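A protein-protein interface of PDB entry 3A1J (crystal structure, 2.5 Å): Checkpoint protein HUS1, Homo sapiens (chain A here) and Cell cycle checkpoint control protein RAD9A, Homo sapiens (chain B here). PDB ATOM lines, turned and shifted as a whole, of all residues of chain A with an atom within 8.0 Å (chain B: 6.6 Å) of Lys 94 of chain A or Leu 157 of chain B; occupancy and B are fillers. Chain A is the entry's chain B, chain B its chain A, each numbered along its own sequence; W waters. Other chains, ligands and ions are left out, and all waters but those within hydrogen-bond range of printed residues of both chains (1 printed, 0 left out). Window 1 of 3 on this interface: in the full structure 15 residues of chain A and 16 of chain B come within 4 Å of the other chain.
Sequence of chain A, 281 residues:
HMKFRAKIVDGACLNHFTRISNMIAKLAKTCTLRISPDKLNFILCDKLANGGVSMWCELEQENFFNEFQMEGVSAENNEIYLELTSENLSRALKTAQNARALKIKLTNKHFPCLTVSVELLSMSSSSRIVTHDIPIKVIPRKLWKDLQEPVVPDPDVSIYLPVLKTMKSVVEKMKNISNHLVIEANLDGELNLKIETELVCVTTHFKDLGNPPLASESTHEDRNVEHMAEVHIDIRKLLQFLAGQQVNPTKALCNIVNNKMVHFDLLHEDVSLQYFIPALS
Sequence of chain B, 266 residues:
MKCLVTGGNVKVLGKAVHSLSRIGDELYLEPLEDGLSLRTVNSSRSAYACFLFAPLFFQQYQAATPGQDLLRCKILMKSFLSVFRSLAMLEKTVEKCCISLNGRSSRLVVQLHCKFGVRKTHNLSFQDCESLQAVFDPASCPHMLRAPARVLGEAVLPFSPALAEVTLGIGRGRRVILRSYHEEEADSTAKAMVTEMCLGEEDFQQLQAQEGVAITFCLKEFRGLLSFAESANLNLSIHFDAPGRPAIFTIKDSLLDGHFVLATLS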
ATOM      1  N   THR A  18      -9.414  -9.641 -40.750  1.00  0.00           N
ATOM      2  CA  THR A  18      -8.774 -10.059 -39.514  1.00  0.00           C
ATOM      3  C   THR A  18      -7.276  -9.781 -39.536  1.00  0.00           C
ATOM      4  O   THR A  18      -6.696  -9.350 -38.537  1.00  0.00           O
ATOM      5  CB  THR A  18      -9.000 -11.559 -39.283  1.00  0.00           C
ATOM      6  OG1 THR A  18     -10.401 -11.803 -39.105  1.00  0.00           O
ATOM      7  CG2 THR A  18      -8.232 -12.043 -38.062  1.00  0.00           C
ATOM      8  N   SER A  21      -6.673  -6.126 -39.198  1.00  0.00           N
ATOM      9  CA  SER A  21      -6.885  -5.773 -37.801  1.00  0.00           C
ATOM     10  C   SER A  21      -5.671  -6.163 -36.950  1.00  0.00           C
ATOM     11  O   SER A  21      -5.265  -5.412 -36.062  1.00  0.00           O
ATOM     12  CB  SER A  21      -8.134  -6.482 -37.284  1.00  0.00           C
ATOM     13  OG  SER A  21      -8.012  -6.804 -35.913  1.00  0.00           O
ATOM     14  N   ASN A  22      -5.099  -7.339 -37.203  1.00  0.00           N
ATOM     15  CA  ASN A  22      -3.927  -7.784 -36.446  1.00  0.00           C
ATOM     16  C   ASN A  22      -2.768  -6.847 -36.732  1.00  0.00           C
ATOM     17  O   ASN A  22      -1.926  -6.601 -35.868  1.00  0.00           O
ATOM     18  CB  ASN A  22      -3.496  -9.212 -36.818  1.00  0.00           C
ATOM     19  CG  ASN A  22      -4.497 -10.270 -36.386  1.00  0.00           C
ATOM     20  OD1 ASN A  22      -5.318 -10.053 -35.491  1.00  0.00           O
ATOM     21  ND2 ASN A  22      -4.419 -11.433 -37.017  1.00  0.00           N
ATOM     22  N   GLU A  87      -5.912  -3.835 -29.876  1.00  0.00           N
ATOM     23  CA  GLU A  87      -5.932  -5.245 -29.499  1.00  0.00           C
ATOM     24  C   GLU A  87      -7.369  -5.706 -29.266  1.00  0.00           C
ATOM     25  O   GLU A  87      -7.685  -6.874 -29.448  1.00  0.00           O
ATOM     26  CB  GLU A  87      -5.086  -5.487 -28.246  1.00  0.00           C
ATOM     27  CG  GLU A  87      -5.868  -5.471 -26.956  1.00  0.00           C
ATOM     28  CD  GLU A  87      -6.575  -6.784 -26.680  1.00  0.00           C
ATOM     29  OE1 GLU A  87      -7.610  -6.757 -25.985  1.00  0.00           O
ATOM     30  OE2 GLU A  87      -6.094  -7.839 -27.146  1.00  0.00           O
ATOM     31  N   ASN A  88      -8.237  -4.783 -28.861  1.00  0.00           N
ATOM     32  CA  ASN A  88      -9.632  -5.101 -28.627  1.00  0.00           C
ATOM     33  C   ASN A  88     -10.261  -5.689 -29.895  1.00  0.00           C
ATOM     34  O   ASN A  88     -10.921  -6.724 -29.848  1.00  0.00           O
ATOM     35  CB  ASN A  88     -10.383  -3.839 -28.181  1.00  0.00           C
ATOM     36  CG  ASN A  88     -10.245  -3.572 -26.688  1.00  0.00           C
ATOM     37  OD1 ASN A  88      -9.352  -4.095 -26.037  1.00  0.00           O
ATOM     38  ND2 ASN A  88     -11.129  -2.746 -26.147  1.00  0.00           N
ATOM     39  N   LEU A  89     -10.046  -5.030 -31.026  1.00  0.00           N
ATOM     40  CA  LEU A  89     -10.588  -5.492 -32.291  1.00  0.00           C
ATOM     41  C   LEU A  89      -9.932  -6.790 -32.772  1.00  0.00           C
ATOM     42  O   LEU A  89     -10.556  -7.581 -33.482  1.00  0.00           O
ATOM     43  CB  LEU A  89     -10.438  -4.408 -33.359  1.00  0.00           C
ATOM     44  CG  LEU A  89     -10.867  -4.836 -34.767  1.00  0.00           C
ATOM     45  CD1 LEU A  89     -12.317  -5.318 -34.735  1.00  0.00           C
ATOM     46  CD2 LEU A  89     -10.706  -3.673 -35.739  1.00  0.00           C
ATOM     47  N   SER A  90      -8.676  -7.008 -32.396  1.00  0.00           N
ATOM     48  CA  SER A  90      -7.984  -8.230 -32.786  1.00  0.00           C
ATOM     49  C   SER A  90      -8.491  -9.388 -31.944  1.00  0.00           C
ATOM     50  O   SER A  90      -8.719 -10.480 -32.465  1.00  0.00           O
ATOM     51  CB  SER A  90      -6.478  -8.108 -32.569  1.00  0.00           C
ATOM     52  OG  SER A  90      -5.927  -7.085 -33.372  1.00  0.00           O
ATOM     53  N   ARG A  91      -8.657  -9.155 -30.644  1.00  0.00           N
ATOM     54  CA  ARG A  91      -9.132 -10.205 -29.758  1.00  0.00           C
ATOM     55  C   ARG A  91     -10.525 -10.633 -30.177  1.00  0.00           C
ATOM     56  O   ARG A  91     -10.873 -11.809 -30.084  1.00  0.00           O
ATOM     57  CB  ARG A  91      -9.157  -9.746 -28.301  1.00  0.00           C
ATOM     58  CG  ARG A  91      -9.069 -10.921 -27.331  1.00  0.00           C
ATOM     59  CD  ARG A  91      -9.507 -10.564 -25.938  1.00  0.00           C
ATOM     60  NE  ARG A  91      -8.962  -9.288 -25.490  1.00  0.00           N
ATOM     61  CZ  ARG A  91      -9.348  -8.681 -24.376  1.00  0.00           C
ATOM     62  NH1 ARG A  91     -10.268  -9.249 -23.610  1.00  0.00           N
ATOM     63  NH2 ARG A  91      -8.865  -7.490 -24.050  1.00  0.00           N
ATOM     64  N   ALA A  92     -11.317  -9.679 -30.657  1.00  0.00           N
ATOM     65  CA  ALA A  92     -12.666  -9.976 -31.101  1.00  0.00           C
ATOM     66  C   ALA A  92     -12.646 -10.879 -32.351  1.00  0.00           C
ATOM     67  O   ALA A  92     -13.489 -11.761 -32.505  1.00  0.00           O
ATOM     68  CB  ALA A  92     -13.402  -8.681 -31.396  1.00  0.00           C
ATOM     69  N   LEU A  93     -11.676 -10.667 -33.237  1.00  0.00           N
ATOM     70  CA  LEU A  93     -11.580 -11.459 -34.456  1.00  0.00           C
ATOM     71  C   LEU A  93     -10.787 -12.750 -34.246  1.00  0.00           C
ATOM     72  O   LEU A  93     -10.530 -13.501 -35.182  1.00  0.00           O
ATOM     73  CB  LEU A  93     -10.930 -10.625 -35.549  1.00  0.00           C
ATOM     74  CG  LEU A  93     -11.603  -9.277 -35.807  1.00  0.00           C
ATOM     75  CD1 LEU A  93     -10.807  -8.490 -36.839  1.00  0.00           C
ATOM     76  CD2 LEU A  93     -13.021  -9.501 -36.283  1.00  0.00           C
ATOM     77  N   LYS A  94     -10.423 -12.996 -32.995  1.00  0.00           N
ATOM     78  CA  LYS A  94      -9.649 -14.160 -32.586  1.00  0.00           C
ATOM     79  C   LYS A  94     -10.110 -15.508 -33.138  1.00  0.00           C
ATOM     80  O   LYS A  94      -9.276 -16.324 -33.546  1.00  0.00           O
ATOM     81  CB  LYS A  94      -9.628 -14.215 -31.054  1.00  0.00           C
ATOM     82  CG  LYS A  94      -8.751 -15.286 -30.421  1.00  0.00           C
ATOM     83  CD  LYS A  94      -8.846 -15.184 -28.897  1.00  0.00           C
ATOM     84  CE  LYS A  94      -7.970 -16.196 -28.171  1.00  0.00           C
ATOM     85  NZ  LYS A  94      -7.885 -15.873 -26.710  1.00  0.00           N
ATOM     86  N   THR A  95     -11.420 -15.755 -33.150  1.00  0.00           N
ATOM     87  CA  THR A  95     -11.931 -17.042 -33.626  1.00  0.00           C
ATOM     88  C   THR A  95     -12.565 -17.020 -35.006  1.00  0.00           C
ATOM     89  O   THR A  95     -13.212 -17.984 -35.408  1.00  0.00           O
ATOM     90  CB  THR A  95     -12.973 -17.620 -32.657  1.00  0.00           C
ATOM     91  OG1 THR A  95     -14.049 -16.689 -32.510  1.00  0.00           O
ATOM     92  CG2 THR A  95     -12.355 -17.891 -31.297  1.00  0.00           C
ATOM     93  N   ALA A  96     -12.366 -15.930 -35.735  1.00  0.00           N
ATOM     94  CA  ALA A  96     -12.935 -15.767 -37.070  1.00  0.00           C
ATOM     95  C   ALA A  96     -12.423 -16.804 -38.080  1.00  0.00           C
ATOM     96  O   ALA A  96     -12.942 -16.916 -39.193  1.00  0.00           O
ATOM     97  CB  ALA A  96     -12.656 -14.351 -37.569  1.00  0.00           C
ATOM     98  N   GLN A  97     -11.409 -17.564 -37.682  1.00  0.00           N
ATOM     99  CA  GLN A  97     -10.825 -18.599 -38.536  1.00  0.00           C
ATOM    100  C   GLN A  97     -11.870 -19.672 -38.834  1.00  0.00           C
ATOM    101  O   GLN A  97     -11.904 -20.255 -39.923  1.00  0.00           O
ATOM    102  CB  GLN A  97      -9.639 -19.253 -37.818  1.00  0.00           C
ATOM    103  CG  GLN A  97     -10.024 -19.823 -36.453  1.00  0.00           C
ATOM    104  CD  GLN A  97      -8.940 -20.673 -35.820  1.00  0.00           C
ATOM    105  OE1 GLN A  97      -8.448 -21.626 -36.428  1.00  0.00           O
ATOM    106  NE2 GLN A  97      -8.573 -20.341 -34.581  1.00  0.00           N
ATOM    107  N   ASN A  98     -12.710 -19.937 -37.841  1.00  0.00           N
ATOM    108  CA  ASN A  98     -13.754 -20.944 -37.964  1.00  0.00           C
ATOM    109  C   ASN A  98     -15.089 -20.232 -37.976  1.00  0.00           C
ATOM    110  O   ASN A  98     -16.054 -20.708 -37.380  1.00  0.00           O
ATOM    111  CB  ASN A  98     -13.709 -21.905 -36.772  1.00  0.00           C
ATOM    112  CG  ASN A  98     -12.377 -22.626 -36.651  1.00  0.00           C
ATOM    113  OD1 ASN A  98     -11.998 -23.411 -37.525  1.00  0.00           O
ATOM    114  ND2 ASN A  98     -11.658 -22.362 -35.563  1.00  0.00           N
ATOM    115  N   LEU A 102     -19.642 -12.629 -39.889  1.00  0.00           N
ATOM    116  CA  LEU A 102     -19.218 -11.630 -38.931  1.00  0.00           C
ATOM    117  C   LEU A 102     -20.149 -10.434 -39.028  1.00  0.00           C
ATOM    118  O   LEU A 102     -20.483  -9.989 -40.129  1.00  0.00           O
ATOM    119  CB  LEU A 102     -17.795 -11.167 -39.233  1.00  0.00           C
ATOM    120  CG  LEU A 102     -17.296 -10.069 -38.287  1.00  0.00           C
ATOM    121  CD1 LEU A 102     -16.930 -10.717 -36.966  1.00  0.00           C
ATOM    122  CD2 LEU A 102     -16.085  -9.335 -38.869  1.00  0.00           C
ATOM    123  N   VAL A 116     -19.055  -6.695 -32.001  1.00  0.00           N
ATOM    124  CA  VAL A 116     -18.693  -7.652 -33.049  1.00  0.00           C
ATOM    125  C   VAL A 116     -19.209  -9.041 -32.716  1.00  0.00           C
ATOM    126  O   VAL A 116     -18.863  -9.610 -31.681  1.00  0.00           O
ATOM    127  CB  VAL A 116     -17.175  -7.725 -33.221  1.00  0.00           C
ATOM    128  CG1 VAL A 116     -16.810  -8.842 -34.185  1.00  0.00           C
ATOM    129  CG2 VAL A 116     -16.664  -6.393 -33.728  1.00  0.00           C
ATOM    130  N   VAL A 118     -19.418 -12.962 -33.886  1.00  0.00           N
ATOM    131  CA  VAL A 118     -18.883 -13.982 -34.778  1.00  0.00           C
ATOM    132  C   VAL A 118     -19.752 -15.230 -34.742  1.00  0.00           C
ATOM    133  O   VAL A 118     -19.851 -15.893 -33.720  1.00  0.00           O
ATOM    134  CB  VAL A 118     -17.450 -14.367 -34.384  1.00  0.00           C
ATOM    135  CG1 VAL A 118     -16.823 -15.211 -35.478  1.00  0.00           C
ATOM    136  CG2 VAL A 118     -16.628 -13.117 -34.133  1.00  0.00           C
ATOM    137  N   LEU A 120     -20.032 -18.761 -35.454  1.00  0.00           N
ATOM    138  CA  LEU A 120     -19.140 -19.877 -35.744  1.00  0.00           C
ATOM    139  C   LEU A 120     -19.743 -20.914 -36.687  1.00  0.00           C
ATOM    140  O   LEU A 120     -20.961 -21.076 -36.769  1.00  0.00           O
ATOM    141  CB  LEU A 120     -18.699 -20.560 -34.444  1.00  0.00           C
ATOM    142  CG  LEU A 120     -18.034 -19.665 -33.388  1.00  0.00           C
ATOM    143  CD1 LEU A 120     -17.611 -20.512 -32.191  1.00  0.00           C
ATOM    144  CD2 LEU A 120     -16.828 -18.953 -33.986  1.00  0.00           C
ATOM    145  N   VAL A 130     -20.211 -15.786 -30.807  1.00  0.00           N
ATOM    146  CA  VAL A 130     -19.267 -15.087 -29.944  1.00  0.00           C
ATOM    147  C   VAL A 130     -19.568 -13.590 -30.071  1.00  0.00           C
ATOM    148  O   VAL A 130     -19.498 -13.032 -31.167  1.00  0.00           O
ATOM    149  CB  VAL A 130     -17.792 -15.322 -30.388  1.00  0.00           C
ATOM    150  CG1 VAL A 130     -16.834 -14.758 -29.340  1.00  0.00           C
ATOM    151  CG2 VAL A 130     -17.539 -16.801 -30.609  1.00  0.00           C
ATOM    152  N   HIS A 132     -18.700  -9.631 -28.736  1.00  0.00           N
ATOM    153  CA  HIS A 132     -17.712  -8.762 -28.087  1.00  0.00           C
ATOM    154  C   HIS A 132     -18.188  -7.303 -28.119  1.00  0.00           C
ATOM    155  O   HIS A 132     -18.542  -6.774 -29.184  1.00  0.00           O
ATOM    156  CB  HIS A 132     -16.388  -8.821 -28.834  1.00  0.00           C
ATOM    157  CG  HIS A 132     -15.796 -10.191 -28.935  1.00  0.00           C
ATOM    158  ND1 HIS A 132     -14.922 -10.696 -27.997  1.00  0.00           N
ATOM    159  CD2 HIS A 132     -15.899 -11.134 -29.901  1.00  0.00           C
ATOM    160  CE1 HIS A 132     -14.504 -11.888 -28.382  1.00  0.00           C
ATOM    161  NE2 HIS A 132     -15.082 -12.178 -29.535  1.00  0.00           N
ATOM    162  N   LEU B 152     -16.147 -27.840 -23.830  1.00  0.00           N
ATOM    163  CA  LEU B 152     -16.072 -26.712 -22.911  1.00  0.00           C
ATOM    164  C   LEU B 152     -14.795 -25.946 -23.199  1.00  0.00           C
ATOM    165  O   LEU B 152     -14.736 -24.732 -23.036  1.00  0.00           O
ATOM    166  CB  LEU B 152     -16.091 -27.204 -21.462  1.00  0.00           C
ATOM    167  CG  LEU B 152     -17.369 -27.963 -21.120  1.00  0.00           C
ATOM    168  CD1 LEU B 152     -17.377 -28.421 -19.673  1.00  0.00           C
ATOM    169  CD2 LEU B 152     -18.537 -27.050 -21.394  1.00  0.00           C
ATOM    170  N   GLY B 153     -13.770 -26.673 -23.637  1.00  0.00           N
ATOM    171  CA  GLY B 153     -12.503 -26.044 -23.956  1.00  0.00           C
ATOM    172  C   GLY B 153     -12.720 -25.052 -25.079  1.00  0.00           C
ATOM    173  O   GLY B 153     -12.127 -23.968 -25.089  1.00  0.00           O
ATOM    174  N   GLU B 154     -13.581 -25.425 -26.027  1.00  0.00           N
ATOM    175  CA  GLU B 154     -13.894 -24.562 -27.155  1.00  0.00           C
ATOM    176  C   GLU B 154     -14.768 -23.406 -26.666  1.00  0.00           C
ATOM    177  O   GLU B 154     -14.667 -22.288 -27.166  1.00  0.00           O
ATOM    178  CB  GLU B 154     -14.620 -25.359 -28.247  1.00  0.00           C
ATOM    179  CG  GLU B 154     -13.756 -26.436 -28.891  1.00  0.00           C
ATOM    180  CD  GLU B 154     -14.516 -27.350 -29.857  1.00  0.00           C
ATOM    181  OE1 GLU B 154     -13.875 -28.253 -30.444  1.00  0.00           O
ATOM    182  OE2 GLU B 154     -15.746 -27.183 -30.028  1.00  0.00           O
ATOM    183  N   ALA B 155     -15.605 -23.679 -25.669  1.00  0.00           N
ATOM    184  CA  ALA B 155     -16.491 -22.662 -25.106  1.00  0.00           C
ATOM    185  C   ALA B 155     -15.704 -21.537 -24.432  1.00  0.00           C
ATOM    186  O   ALA B 155     -16.096 -20.372 -24.462  1.00  0.00           O
ATOM    187  CB  ALA B 155     -17.439 -23.307 -24.102  1.00  0.00           C
ATOM    188  N   VAL B 156     -14.579 -21.905 -23.839  1.00  0.00           N
ATOM    189  CA  VAL B 156     -13.716 -20.974 -23.123  1.00  0.00           C
ATOM    190  C   VAL B 156     -12.608 -20.348 -23.991  1.00  0.00           C
ATOM    191  O   VAL B 156     -11.904 -19.431 -23.563  1.00  0.00           O
ATOM    192  CB  VAL B 156     -13.106 -21.716 -21.906  1.00  0.00           C
ATOM    193  CG1 VAL B 156     -12.057 -20.874 -21.221  1.00  0.00           C
ATOM    194  CG2 VAL B 156     -14.222 -22.078 -20.930  1.00  0.00           C
ATOM    195  N   LEU B 157     -12.475 -20.819 -25.223  1.00  0.00           N
ATOM    196  CA  LEU B 157     -11.439 -20.314 -26.122  1.00  0.00           C
ATOM    197  C   LEU B 157     -11.473 -18.817 -26.448  1.00  0.00           C
ATOM    198  O   LEU B 157     -10.425 -18.179 -26.522  1.00  0.00           O
ATOM    199  CB  LEU B 157     -11.472 -21.100 -27.424  1.00  0.00           C
ATOM    200  CG  LEU B 157     -10.242 -21.046 -28.318  1.00  0.00           C
ATOM    201  CD1 LEU B 157      -9.065 -21.721 -27.633  1.00  0.00           C
ATOM    202  CD2 LEU B 157     -10.567 -21.756 -29.621  1.00  0.00           C
ATOM    203  N   PRO B 158     -12.668 -18.231 -26.646  1.00  0.00           N
ATOM    204  CA  PRO B 158     -12.768 -16.798 -26.972  1.00  0.00           C
ATOM    205  C   PRO B 158     -12.243 -15.832 -25.899  1.00  0.00           C
ATOM    206  O   PRO B 158     -11.812 -14.719 -26.206  1.00  0.00           O
ATOM    207  CB  PRO B 158     -14.264 -16.596 -27.208  1.00  0.00           C
ATOM    208  CG  PRO B 158     -14.768 -17.959 -27.570  1.00  0.00           C
ATOM    209  CD  PRO B 158     -14.003 -18.853 -26.635  1.00  0.00           C
ATOM    210  N   PHE B 159     -12.287 -16.255 -24.642  1.00  0.00           N
ATOM    211  CA  PHE B 159     -11.849 -15.401 -23.552  1.00  0.00           C
ATOM    212  C   PHE B 159     -10.341 -15.297 -23.511  1.00  0.00           C
ATOM    213  O   PHE B 159      -9.640 -16.122 -24.094  1.00  0.00           O
ATOM    214  CB  PHE B 159     -12.369 -15.946 -22.220  1.00  0.00           C
ATOM    215  CG  PHE B 159     -13.857 -16.072 -22.172  1.00  0.00           C
ATOM    216  CD1 PHE B 159     -14.666 -14.932 -22.180  1.00  0.00           C
ATOM    217  CD2 PHE B 159     -14.459 -17.324 -22.205  1.00  0.00           C
ATOM    218  CE1 PHE B 159     -16.053 -15.042 -22.231  1.00  0.00           C
ATOM    219  CE2 PHE B 159     -15.838 -17.441 -22.257  1.00  0.00           C
ATOM    220  CZ  PHE B 159     -16.639 -16.298 -22.271  1.00  0.00           C
ATOM    221  N   SER B 160      -9.848 -14.270 -22.826  1.00  0.00           N
ATOM    222  CA  SER B 160      -8.419 -14.063 -22.686  1.00  0.00           C
ATOM    223  C   SER B 160      -7.816 -15.075 -21.724  1.00  0.00           C
ATOM    224  O   SER B 160      -8.426 -15.425 -20.708  1.00  0.00           O
ATOM    225  CB  SER B 160      -8.138 -12.659 -22.155  1.00  0.00           C
ATOM    226  OG  SER B 160      -6.853 -12.608 -21.549  1.00  0.00           O
ATOM    227  N   PRO B 161      -6.600 -15.556 -22.027  1.00  0.00           N
ATOM    228  CA  PRO B 161      -5.903 -16.527 -21.179  1.00  0.00           C
ATOM    229  C   PRO B 161      -5.767 -15.959 -19.777  1.00  0.00           C
ATOM    230  O   PRO B 161      -5.637 -16.700 -18.806  1.00  0.00           O
ATOM    231  CB  PRO B 161      -4.548 -16.656 -21.859  1.00  0.00           C
ATOM    232  CG  PRO B 161      -4.884 -16.470 -23.292  1.00  0.00           C
ATOM    233  CD  PRO B 161      -5.828 -15.292 -23.254  1.00  0.00           C
ATOM    234  N   MET B 197     -20.035 -16.006 -24.944  1.00  0.00           N
ATOM    235  CA  MET B 197     -20.106 -17.159 -25.823  1.00  0.00           C
ATOM    236  C   MET B 197     -21.432 -17.830 -25.560  1.00  0.00           C
ATOM    237  O   MET B 197     -21.739 -18.186 -24.424  1.00  0.00           O
ATOM    238  CB  MET B 197     -18.976 -18.148 -25.549  1.00  0.00           C
ATOM    239  CG  MET B 197     -18.153 -18.449 -26.786  1.00  0.00           C
ATOM    240  SD  MET B 197     -18.880 -19.688 -28.117  1.00  0.00           S
ATOM    241  CE  MET B 197     -20.513 -18.853 -28.577  1.00  0.00           C
ATOM    242  N   ARG B 223      -9.775 -23.867 -15.602  1.00  0.00           N
ATOM    243  CA  ARG B 223      -8.829 -24.261 -16.642  1.00  0.00           C
ATOM    244  C   ARG B 223      -7.856 -25.344 -16.175  1.00  0.00           C
ATOM    245  O   ARG B 223      -7.341 -26.111 -16.984  1.00  0.00           O
ATOM    246  CB  ARG B 223      -8.052 -23.034 -17.130  1.00  0.00           C
ATOM    247  CG  ARG B 223      -8.913 -22.103 -17.955  1.00  0.00           C
ATOM    248  CD  ARG B 223      -8.157 -20.882 -18.436  1.00  0.00           C
ATOM    249  NE  ARG B 223      -8.697 -20.463 -19.724  1.00  0.00           N
ATOM    250  CZ  ARG B 223      -8.796 -19.205 -20.120  1.00  0.00           C
ATOM    251  NH1 ARG B 223      -8.385 -18.226 -19.322  1.00  0.00           N
ATOM    252  NH2 ARG B 223      -9.320 -18.931 -21.308  1.00  0.00           N
HETATM  253  O   HOH W   1     -12.031 -14.007 -28.900  1.00  0.00           O
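Printed residues of chain A within 4 Å of Leu 157 of chain B: Lys 94. Pro 158 of chain B touches just one residue of chain A: Val 130 (3.8 Å). Of the printed residues of chain A, Phe 159 of chain B touches Lys 94. Printed residues of chain A within 4 Å of Met 197 of chain B: Val 130 (3.8 Å). Printed residues of chain B within 4 Å of Val 130 of chain A: Pro 158 (3.8 Å) and Met 197 (3.8 Å). Thr 95 of chain A touches none of the printed residues of chain B. Leu 93 of chain A touches none of the printed residues of chain B.
The backbone NH of Val 118 of chain A lies within hydrogen-bond range of the backbone carbonyl oxygen of Val 130 of chain A (2.7 Å).
Among the printed residues, pairs that only touch across the chains: Val 130 of chain A with Pro 158 of chain B (3.8 Å) and Val 130 of chain A with Met 197 of chain B (3.8 Å).
Of the 12 printed residues of chain B, 4 touch a printed residue of chain A. Hydrophobic or aromatic side chains of chain B that line the printed part of chain A: Pro 158 and Met 197. Printed residues of chain A that touch a printed residue of chain B: Lys 94 and Val 130. Among the printed residues, no Asp or Glu carboxylate lies within 4 Å of a Lys or Arg side-chain nitrogen of the other chain.
The side-chain amino group of Lys 94 of chain A sits at hydrogen-bond distance from the backbone carbonyl oxygen of Leu 157 of chain B, at 3.4 Å. O of Phe 159 of chain B sits at hydrogen-bond distance from NZ of Lys 94 of chain A (3.2 Å).
Water W1 lies within hydrogen-bond range of O of Arg 91 of chain A (2.8 Å) and O of Pro 158 of chain B (2.8 Å).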
